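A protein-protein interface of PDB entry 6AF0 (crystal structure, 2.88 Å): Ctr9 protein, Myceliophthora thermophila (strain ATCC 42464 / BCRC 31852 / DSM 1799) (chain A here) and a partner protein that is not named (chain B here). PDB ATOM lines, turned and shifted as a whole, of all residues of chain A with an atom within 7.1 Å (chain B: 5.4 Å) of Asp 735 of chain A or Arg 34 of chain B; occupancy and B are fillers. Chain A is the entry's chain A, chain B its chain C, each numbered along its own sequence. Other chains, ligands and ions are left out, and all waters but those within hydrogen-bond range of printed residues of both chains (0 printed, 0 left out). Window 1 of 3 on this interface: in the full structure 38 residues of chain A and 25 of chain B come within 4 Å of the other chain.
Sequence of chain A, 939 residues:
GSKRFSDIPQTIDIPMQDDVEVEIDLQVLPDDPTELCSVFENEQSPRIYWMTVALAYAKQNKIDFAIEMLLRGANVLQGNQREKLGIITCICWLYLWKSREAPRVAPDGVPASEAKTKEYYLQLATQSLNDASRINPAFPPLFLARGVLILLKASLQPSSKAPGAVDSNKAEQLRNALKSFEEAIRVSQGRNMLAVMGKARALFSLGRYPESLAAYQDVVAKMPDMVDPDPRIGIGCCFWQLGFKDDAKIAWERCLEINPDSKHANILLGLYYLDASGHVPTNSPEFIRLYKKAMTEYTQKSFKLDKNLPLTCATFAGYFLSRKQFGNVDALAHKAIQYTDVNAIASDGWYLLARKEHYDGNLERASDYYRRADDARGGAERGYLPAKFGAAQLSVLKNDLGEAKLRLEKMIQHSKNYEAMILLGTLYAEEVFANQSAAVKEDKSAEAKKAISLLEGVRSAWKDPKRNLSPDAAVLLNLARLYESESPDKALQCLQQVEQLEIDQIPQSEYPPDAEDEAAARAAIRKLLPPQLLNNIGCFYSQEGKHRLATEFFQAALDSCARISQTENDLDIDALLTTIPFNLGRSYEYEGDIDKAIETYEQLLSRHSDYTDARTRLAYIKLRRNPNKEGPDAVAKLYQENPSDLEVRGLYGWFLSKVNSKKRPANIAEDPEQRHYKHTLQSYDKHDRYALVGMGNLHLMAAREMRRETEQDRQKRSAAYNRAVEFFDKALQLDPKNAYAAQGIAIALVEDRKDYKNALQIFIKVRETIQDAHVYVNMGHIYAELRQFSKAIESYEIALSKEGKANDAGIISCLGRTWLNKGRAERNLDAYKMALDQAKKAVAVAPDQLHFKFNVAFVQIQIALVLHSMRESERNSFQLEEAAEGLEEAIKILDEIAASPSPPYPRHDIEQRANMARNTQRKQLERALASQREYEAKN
The backbone carbonyl oxygen (O) of Lys 37 of chain B is in hydrogen-bond range of the side-chain hydroxyl (OG1) of Thr 769 of chain A.
The backbone carbonyl oxygen (O) of Thr 769 of chain A sits at hydrogen-bond distance from the backbone NH (N) of Ile 36 of chain B (2.9 Å).
N of Arg 689 of chain A is in hydrogen-bond range of OD1 of Asn 30 of chain B (3.1 Å).
The backbone carbonyl oxygen (O) of Pro 736 of chain A lies close to the backbone carbonyl oxygen (O) of Thr 39 of chain B (3.1 Å).
The side-chain carboxylate (OD2) of Asp 735 of chain A is in salt-bridge range of the guanidinium group (NE) of Arg 34 of chain B (2.8 Å).
The backbone NH of Ala 739 of chain A lies within hydrogen-bond range of the backbone carbonyl oxygen of Leu 33 of chain B (2.9 Å).
The side-chain hydroxyl (OG1) of Thr 769 of chain A sits at hydrogen-bond distance from the backbone carbonyl oxygen (O) of Arg 34 of chain B (2.9 Å).
The backbone carbonyl oxygen of Lys 37 of chain B lies within hydrogen-bond range of the side-chain hydroxyl of Thr 39 of chain B (3.2 Å).
OD1 of Asn 738 of chain A sits at hydrogen-bond distance from N of Ala 741 of chain A, 2.7 Å away.
NH1 of Arg 689 of chain A lies within salt-bridge range of OD2 of Asp 735 of chain A, at 3.0 Å.
The side-chain amide oxygen (OD1) of Asn 738 of chain A lies within hydrogen-bond range of the backbone NH (N) of Tyr 740 of chain A (2.9 Å).
Arg 689 of chain A touches Arg 34 of chain B (NH1 to NH2, 3.6 Å).
Lys 737 of chain A touches Arg 34 of chain B.
Lys 737 of chain A touches Pro 38 of chain B (CB to CB, 3.98 Å).
Lys 737 of chain A touches Thr 39 of chain B (CA to O, 2.9 Å).
Leu 33 of chain B touches Asn 738 of chain A.
Leu 33 of chain B touches Tyr 740 of chain A (O to CD2, 3.3 Å).
Thr 769 of chain A touches Gly 35 of chain B.
Ile 770 of chain A touches Gly 35 of chain B.
Asp 729 of chain A touches none of the printed residues of chain B.
Of chain B, only Arg 34 (2.8 Å) comes within 4 Å of Asp 735 of chain A.
Of the printed residues of chain B, Pro 736 of chain A touches Thr 39.
Of the printed residues of chain B, Tyr 740 of chain A touches Leu 33 (3.3 Å).
Ala 741 of chain A touches none of the printed residues of chain B.
Of the printed residues of chain B, Ile 770 of chain A touches Gly 35.
Printed residues of chain A within 4 Å of Pro 38 of chain B: Lys 737.
Of the printed residues of chain A, Thr 39 of chain B touches Pro 736 and Lys 737.
The nearest residue of chain B that does not touch Asp 735 of chain A is Asn 30 of chain B (4.1 Å).
The nearest residue of chain A that does not touch Arg 34 of chain B is Asn 738 of chain A (4.2 Å).
The nearest printed residue of chain B that does not touch Asn 738 of chain A is Arg 34 of chain B (4.2 Å).
Of the 10 printed residues of chain B, 8 touch a printed residue of chain A.
Along chain B the printed residues that touch a printed residue of chain A span positions 30 to 39.
Among the printed residues, Asp or Glu carboxylates within 4 Å of a Lys or Arg side-chain nitrogen of the other chain: Asp 735 of chain A with Arg 34 of chain B (2.8 Å).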
ATOM      1  N   SER A 485      23.575   8.522 -24.101  1.00  0.00           N
ATOM      2  CA  SER A 485      24.067   8.233 -22.763  1.00  0.00           C
ATOM      3  C   SER A 485      22.936   7.883 -21.786  1.00  0.00           C
ATOM      4  O   SER A 485      23.041   6.920 -21.067  1.00  0.00           O
ATOM      5  CB  SER A 485      24.917   9.397 -22.245  1.00  0.00           C
ATOM      6  OG  SER A 485      24.177  10.597 -22.210  1.00  0.00           O
ATOM      7  N   GLU A 486      21.859   8.659 -21.779  1.00  0.00           N
ATOM      8  CA  GLU A 486      20.823   8.565 -20.746  1.00  0.00           C
ATOM      9  C   GLU A 486      19.417   8.347 -21.290  1.00  0.00           C
ATOM     10  O   GLU A 486      18.554   7.861 -20.568  1.00  0.00           O
ATOM     11  CB  GLU A 486      20.866   9.827 -19.877  1.00  0.00           C
ATOM     12  CG  GLU A 486      19.604  10.143 -19.082  1.00  0.00           C
ATOM     13  CD  GLU A 486      19.791  11.324 -18.140  1.00  0.00           C
ATOM     14  OE1 GLU A 486      20.740  11.289 -17.321  1.00  0.00           O
ATOM     15  OE2 GLU A 486      18.988  12.288 -18.219  1.00  0.00           O
ATOM     16  N   ARG A 689      34.159   2.209  -8.900  1.00  0.00           N
ATOM     17  CA  ARG A 689      32.926   1.902  -8.177  1.00  0.00           C
ATOM     18  C   ARG A 689      32.711   0.407  -7.925  1.00  0.00           C
ATOM     19  O   ARG A 689      32.366   0.010  -6.820  1.00  0.00           O
ATOM     20  CB  ARG A 689      31.707   2.465  -8.901  1.00  0.00           C
ATOM     21  CG  ARG A 689      31.522   3.965  -8.717  1.00  0.00           C
ATOM     22  CD  ARG A 689      32.155   4.775  -9.836  1.00  0.00           C
ATOM     23  NE  ARG A 689      31.220   5.006 -10.924  1.00  0.00           N
ATOM     24  CZ  ARG A 689      31.560   5.517 -12.097  1.00  0.00           C
ATOM     25  NH1 ARG A 689      30.635   5.684 -13.026  1.00  0.00           N
ATOM     26  NH2 ARG A 689      32.824   5.854 -12.348  1.00  0.00           N
ATOM     27  N   ASP A 729      29.674   4.822   0.417  1.00  0.00           N
ATOM     28  CA  ASP A 729      29.239   6.206   0.210  1.00  0.00           C
ATOM     29  C   ASP A 729      30.111   6.877  -0.865  1.00  0.00           C
ATOM     30  O   ASP A 729      29.579   7.494  -1.788  1.00  0.00           O
ATOM     31  CB  ASP A 729      29.143   7.000   1.534  1.00  0.00           C
ATOM     32  CG  ASP A 729      30.196   8.081   1.661  1.00  0.00           C
ATOM     33  OD1 ASP A 729      31.388   7.746   1.860  1.00  0.00           O
ATOM     34  OD2 ASP A 729      29.826   9.273   1.551  1.00  0.00           O
ATOM     35  N   LYS A 730      31.430   6.702  -0.790  1.00  0.00           N
ATOM     36  CA  LYS A 730      32.306   7.266  -1.823  1.00  0.00           C
ATOM     37  C   LYS A 730      31.852   6.782  -3.199  1.00  0.00           C
ATOM     38  O   LYS A 730      31.641   7.583  -4.097  1.00  0.00           O
ATOM     39  CB  LYS A 730      33.788   6.914  -1.600  1.00  0.00           C
ATOM     40  CG  LYS A 730      34.759   7.755  -2.446  1.00  0.00           C
ATOM     41  CD  LYS A 730      35.381   8.925  -1.669  1.00  0.00           C
ATOM     42  CE  LYS A 730      36.324   9.782  -2.520  1.00  0.00           C
ATOM     43  NZ  LYS A 730      36.570  11.144  -1.950  1.00  0.00           N
ATOM     44  N   ALA A 731      31.703   5.465  -3.342  1.00  0.00           N
ATOM     45  CA  ALA A 731      31.180   4.842  -4.559  1.00  0.00           C
ATOM     46  C   ALA A 731      29.874   5.501  -5.030  1.00  0.00           C
ATOM     47  O   ALA A 731      29.725   5.854  -6.212  1.00  0.00           O
ATOM     48  CB  ALA A 731      30.947   3.359  -4.314  1.00  0.00           C
ATOM     49  N   LEU A 732      28.931   5.651  -4.097  1.00  0.00           N
ATOM     50  CA  LEU A 732      27.591   6.168  -4.408  1.00  0.00           C
ATOM     51  C   LEU A 732      27.557   7.689  -4.584  1.00  0.00           C
ATOM     52  O   LEU A 732      26.613   8.253  -5.158  1.00  0.00           O
ATOM     53  CB  LEU A 732      26.592   5.747  -3.325  1.00  0.00           C
ATOM     54  CG  LEU A 732      25.125   6.181  -3.487  1.00  0.00           C
ATOM     55  CD1 LEU A 732      24.595   5.901  -4.883  1.00  0.00           C
ATOM     56  CD2 LEU A 732      24.254   5.485  -2.460  1.00  0.00           C
ATOM     57  N   GLN A 733      28.590   8.362  -4.099  1.00  0.00           N
ATOM     58  CA  GLN A 733      28.720   9.795  -4.352  1.00  0.00           C
ATOM     59  C   GLN A 733      29.225  10.077  -5.771  1.00  0.00           C
ATOM     60  O   GLN A 733      28.848  11.075  -6.383  1.00  0.00           O
ATOM     61  CB  GLN A 733      29.618  10.463  -3.308  1.00  0.00           C
ATOM     62  CG  GLN A 733      31.019  10.832  -3.765  1.00  0.00           C
ATOM     63  CD  GLN A 733      31.761  11.625  -2.712  1.00  0.00           C
ATOM     64  OE1 GLN A 733      31.314  11.726  -1.562  1.00  0.00           O
ATOM     65  NE2 GLN A 733      32.892  12.206  -3.099  1.00  0.00           N
ATOM     66  N   LEU A 734      30.075   9.193  -6.286  1.00  0.00           N
ATOM     67  CA  LEU A 734      30.562   9.302  -7.654  1.00  0.00           C
ATOM     68  C   LEU A 734      29.410   8.971  -8.587  1.00  0.00           C
ATOM     69  O   LEU A 734      29.321   9.525  -9.671  1.00  0.00           O
ATOM     70  CB  LEU A 734      31.748   8.358  -7.889  1.00  0.00           C
ATOM     71  CG  LEU A 734      32.858   8.540  -6.854  1.00  0.00           C
ATOM     72  CD1 LEU A 734      33.874   7.410  -6.854  1.00  0.00           C
ATOM     73  CD2 LEU A 734      33.535   9.884  -7.060  1.00  0.00           C
ATOM     74  N   ASP A 735      28.526   8.081  -8.150  1.00  0.00           N
ATOM     75  CA  ASP A 735      27.474   7.573  -9.010  1.00  0.00           C
ATOM     76  C   ASP A 735      26.157   7.395  -8.243  1.00  0.00           C
ATOM     77  O   ASP A 735      25.768   6.281  -7.904  1.00  0.00           O
ATOM     78  CB  ASP A 735      27.930   6.259  -9.652  1.00  0.00           C
ATOM     79  CG  ASP A 735      27.356   6.056 -11.024  1.00  0.00           C
ATOM     80  OD1 ASP A 735      26.358   6.743 -11.368  1.00  0.00           O
ATOM     81  OD2 ASP A 735      27.912   5.189 -11.746  1.00  0.00           O
ATOM     82  N   PRO A 736      25.444   8.501  -8.001  1.00  0.00           N
ATOM     83  CA  PRO A 736      24.170   8.463  -7.310  1.00  0.00           C
ATOM     84  C   PRO A 736      23.178   7.439  -7.867  1.00  0.00           C
ATOM     85  O   PRO A 736      22.186   7.131  -7.207  1.00  0.00           O
ATOM     86  CB  PRO A 736      23.627   9.878  -7.511  1.00  0.00           C
ATOM     87  CG  PRO A 736      24.830  10.723  -7.716  1.00  0.00           C
ATOM     88  CD  PRO A 736      25.781   9.858  -8.463  1.00  0.00           C
ATOM     89  N   LYS A 737      23.437   6.913  -9.061  1.00  0.00           N
ATOM     90  CA  LYS A 737      22.520   5.958  -9.690  1.00  0.00           C
ATOM     91  C   LYS A 737      22.833   4.513  -9.276  1.00  0.00           C
ATOM     92  O   LYS A 737      22.076   3.597  -9.610  1.00  0.00           O
ATOM     93  CB  LYS A 737      22.545   6.099 -11.213  1.00  0.00           C
ATOM     94  CG  LYS A 737      22.310   7.519 -11.714  1.00  0.00           C
ATOM     95  CD  LYS A 737      23.606   8.310 -11.877  1.00  0.00           C
ATOM     96  CE  LYS A 737      23.346   9.806 -11.986  1.00  0.00           C
ATOM     97  NZ  LYS A 737      24.597  10.599 -12.155  1.00  0.00           N
ATOM     98  N   ASN A 738      23.945   4.339  -8.552  1.00  0.00           N
ATOM     99  CA  ASN A 738      24.416   3.045  -8.067  1.00  0.00           C
ATOM    100  C   ASN A 738      23.516   2.392  -7.015  1.00  0.00           C
ATOM    101  O   ASN A 738      23.461   2.805  -5.854  1.00  0.00           O
ATOM    102  CB  ASN A 738      25.824   3.201  -7.497  1.00  0.00           C
ATOM    103  CG  ASN A 738      26.452   1.875  -7.112  1.00  0.00           C
ATOM    104  OD1 ASN A 738      25.811   1.018  -6.473  1.00  0.00           O
ATOM    105  ND2 ASN A 738      27.723   1.702  -7.480  1.00  0.00           N
ATOM    106  N   ALA A 739      22.859   1.319  -7.411  1.00  0.00           N
ATOM    107  CA  ALA A 739      21.880   0.673  -6.555  1.00  0.00           C
ATOM    108  C   ALA A 739      22.530  -0.277  -5.539  1.00  0.00           C
ATOM    109  O   ALA A 739      22.033  -0.441  -4.420  1.00  0.00           O
ATOM    110  CB  ALA A 739      20.898  -0.070  -7.424  1.00  0.00           C
ATOM    111  N   TYR A 740      23.656  -0.874  -5.926  1.00  0.00           N
ATOM    112  CA  TYR A 740      24.338  -1.873  -5.095  1.00  0.00           C
ATOM    113  C   TYR A 740      24.949  -1.254  -3.858  1.00  0.00           C
ATOM    114  O   TYR A 740      24.927  -1.845  -2.779  1.00  0.00           O
ATOM    115  CB  TYR A 740      25.407  -2.650  -5.905  1.00  0.00           C
ATOM    116  CG  TYR A 740      24.777  -3.608  -6.906  1.00  0.00           C
ATOM    117  CD1 TYR A 740      24.568  -4.945  -6.599  1.00  0.00           C
ATOM    118  CD2 TYR A 740      24.320  -3.148  -8.126  1.00  0.00           C
ATOM    119  CE1 TYR A 740      23.926  -5.785  -7.490  1.00  0.00           C
ATOM    120  CE2 TYR A 740      23.702  -3.987  -9.028  1.00  0.00           C
ATOM    121  CZ  TYR A 740      23.494  -5.296  -8.701  1.00  0.00           C
ATOM    122  OH  TYR A 740      22.878  -6.116  -9.612  1.00  0.00           O
ATOM    123  N   ALA A 741      25.486  -0.053  -4.025  1.00  0.00           N
ATOM    124  CA  ALA A 741      26.076   0.692  -2.910  1.00  0.00           C
ATOM    125  C   ALA A 741      25.014   1.143  -1.910  1.00  0.00           C
ATOM    126  O   ALA A 741      25.205   1.034  -0.709  1.00  0.00           O
ATOM    127  CB  ALA A 741      26.837   1.897  -3.443  1.00  0.00           C
ATOM    128  N   THR A 769      15.051  -1.410  -9.739  1.00  0.00           N
ATOM    129  CA  THR A 769      16.241  -1.294 -10.616  1.00  0.00           C
ATOM    130  C   THR A 769      17.162  -2.525 -10.701  1.00  0.00           C
ATOM    131  O   THR A 769      17.974  -2.585 -11.617  1.00  0.00           O
ATOM    132  CB  THR A 769      17.112  -0.041 -10.302  1.00  0.00           C
ATOM    133  OG1 THR A 769      18.106   0.120 -11.317  1.00  0.00           O
ATOM    134  CG2 THR A 769      17.820  -0.139  -8.961  1.00  0.00           C
ATOM    135  N   ILE A 770      17.048  -3.493  -9.790  1.00  0.00           N
ATOM    136  CA  ILE A 770      18.012  -4.601  -9.756  1.00  0.00           C
ATOM    137  C   ILE A 770      17.453  -5.934 -10.239  1.00  0.00           C
ATOM    138  O   ILE A 770      18.007  -6.512 -11.180  1.00  0.00           O
ATOM    139  CB  ILE A 770      18.676  -4.746  -8.377  1.00  0.00           C
ATOM    140  CG1 ILE A 770      19.546  -3.529  -8.084  1.00  0.00           C
ATOM    141  CG2 ILE A 770      19.562  -5.978  -8.307  1.00  0.00           C
ATOM    142  CD1 ILE A 770      20.479  -3.125  -9.210  1.00  0.00           C
ATOM    143  N   ASN B  30      31.059  -0.126 -13.731  1.00  0.00           N
ATOM    144  CA  ASN B  30      30.391   0.811 -12.853  1.00  0.00           C
ATOM    145  C   ASN B  30      28.944   1.062 -13.251  1.00  0.00           C
ATOM    146  O   ASN B  30      28.047   1.129 -12.400  1.00  0.00           O
ATOM    147  CB  ASN B  30      31.156   2.123 -12.839  1.00  0.00           C
ATOM    148  CG  ASN B  30      32.636   1.939 -12.554  1.00  0.00           C
ATOM    149  OD1 ASN B  30      33.031   1.191 -11.653  1.00  0.00           O
ATOM    150  ND2 ASN B  30      33.465   2.629 -13.320  1.00  0.00           N
ATOM    151  N   THR B  31      28.725   1.222 -14.548  1.00  0.00           N
ATOM    152  CA  THR B  31      27.401   1.488 -15.084  1.00  0.00           C
ATOM    153  C   THR B  31      26.482   0.314 -14.866  1.00  0.00           C
ATOM    154  O   THR B  31      25.277   0.484 -14.860  1.00  0.00           O
ATOM    155  CB  THR B  31      27.504   1.741 -16.581  1.00  0.00           C
ATOM    156  OG1 THR B  31      28.320   2.893 -16.757  1.00  0.00           O
ATOM    157  CG2 THR B  31      26.127   1.939 -17.264  1.00  0.00           C
ATOM    158  N   ALA B  32      27.056  -0.880 -14.733  1.00  0.00           N
ATOM    159  CA  ALA B  32      26.277  -2.080 -14.449  1.00  0.00           C
ATOM    160  C   ALA B  32      25.586  -1.983 -13.107  1.00  0.00           C
ATOM    161  O   ALA B  32      24.454  -2.424 -12.969  1.00  0.00           O
ATOM    162  CB  ALA B  32      27.154  -3.310 -14.476  1.00  0.00           C
ATOM    163  N   LEU B  33      26.263  -1.380 -12.135  1.00  0.00           N
ATOM    164  CA  LEU B  33      25.725  -1.262 -10.788  1.00  0.00           C
ATOM    165  C   LEU B  33      24.544  -0.295 -10.674  1.00  0.00           C
ATOM    166  O   LEU B  33      23.881  -0.239  -9.645  1.00  0.00           O
ATOM    167  CB  LEU B  33      26.833  -0.860  -9.833  1.00  0.00           C
ATOM    168  CG  LEU B  33      27.982  -1.866  -9.769  1.00  0.00           C
ATOM    169  CD1 LEU B  33      29.284  -1.202 -10.106  1.00  0.00           C
ATOM    170  CD2 LEU B  33      28.135  -2.459  -8.398  1.00  0.00           C
ATOM    171  N   ARG B  34      24.291   0.469 -11.725  1.00  0.00           N
ATOM    172  CA  ARG B  34      23.152   1.387 -11.763  1.00  0.00           C
ATOM    173  C   ARG B  34      21.886   0.610 -12.064  1.00  0.00           C
ATOM    174  O   ARG B  34      20.773   1.095 -11.832  1.00  0.00           O
ATOM    175  CB  ARG B  34      23.341   2.480 -12.827  1.00  0.00           C
ATOM    176  CG  ARG B  34      24.634   3.272 -12.705  1.00  0.00           C
ATOM    177  CD  ARG B  34      24.719   4.320 -13.797  1.00  0.00           C
ATOM    178  NE  ARG B  34      25.986   5.044 -13.743  1.00  0.00           N
ATOM    179  CZ  ARG B  34      26.297   6.063 -14.529  1.00  0.00           C
ATOM    180  NH1 ARG B  34      25.441   6.481 -15.450  1.00  0.00           N
ATOM    181  NH2 ARG B  34      27.465   6.657 -14.403  1.00  0.00           N
ATOM    182  N   GLY B  35      22.057  -0.589 -12.604  1.00  0.00           N
ATOM    183  CA  GLY B  35      20.944  -1.511 -12.756  1.00  0.00           C
ATOM    184  C   GLY B  35      20.243  -1.335 -14.075  1.00  0.00           C
ATOM    185  O   GLY B  35      20.770  -0.692 -14.951  1.00  0.00           O
ATOM    186  N   ILE B  36      19.048  -1.905 -14.192  1.00  0.00           N
ATOM    187  CA  ILE B  36      18.258  -1.909 -15.431  1.00  0.00           C
ATOM    188  C   ILE B  36      17.605  -0.560 -15.756  1.00  0.00           C
ATOM    189  O   ILE B  36      17.371  -0.252 -16.932  1.00  0.00           O
ATOM    190  CB  ILE B  36      17.146  -2.983 -15.368  1.00  0.00           C
ATOM    191  CG1 ILE B  36      16.612  -3.293 -16.770  1.00  0.00           C
ATOM    192  CG2 ILE B  36      16.010  -2.559 -14.429  1.00  0.00           C
ATOM    193  CD1 ILE B  36      16.179  -4.732 -16.948  1.00  0.00           C
ATOM    194  N   LYS B  37      17.275   0.213 -14.719  1.00  0.00           N
ATOM    195  CA  LYS B  37      16.876   1.620 -14.875  1.00  0.00           C
ATOM    196  C   LYS B  37      17.451   2.489 -13.747  1.00  0.00           C
ATOM    197  O   LYS B  37      16.976   2.405 -12.604  1.00  0.00           O
ATOM    198  CB  LYS B  37      15.349   1.775 -14.923  1.00  0.00           C
ATOM    199  CG  LYS B  37      14.822   3.196 -14.670  1.00  0.00           C
ATOM    200  CD  LYS B  37      15.537   4.294 -15.469  1.00  0.00           C
ATOM    201  CE  LYS B  37      14.960   5.684 -15.229  1.00  0.00           C
ATOM    202  NZ  LYS B  37      15.249   6.215 -13.865  1.00  0.00           N
ATOM    203  N   PRO B  38      18.445   3.353 -14.076  1.00  0.00           N
ATOM    204  CA  PRO B  38      19.055   4.256 -13.101  1.00  0.00           C
ATOM    205  C   PRO B  38      18.040   4.995 -12.243  1.00  0.00           C
ATOM    206  O   PRO B  38      16.890   5.146 -12.643  1.00  0.00           O
ATOM    207  CB  PRO B  38      19.813   5.250 -13.976  1.00  0.00           C
ATOM    208  CG  PRO B  38      20.186   4.466 -15.182  1.00  0.00           C
ATOM    209  CD  PRO B  38      19.069   3.488 -15.409  1.00  0.00           C
ATOM    210  N   THR B  39      18.481   5.442 -11.072  1.00  0.00           N
ATOM    211  CA  THR B  39      17.630   6.120 -10.093  1.00  0.00           C
ATOM    212  C   THR B  39      18.570   6.920  -9.212  1.00  0.00           C
ATOM    213  O   THR B  39      19.743   6.572  -9.107  1.00  0.00           O
ATOM    214  CB  THR B  39      16.853   5.107  -9.225  1.00  0.00           C
ATOM    215  OG1 THR B  39      16.165   4.173 -10.065  1.00  0.00           O
ATOM    216  CG2 THR B  39      15.844   5.801  -8.324  1.00  0.00           C
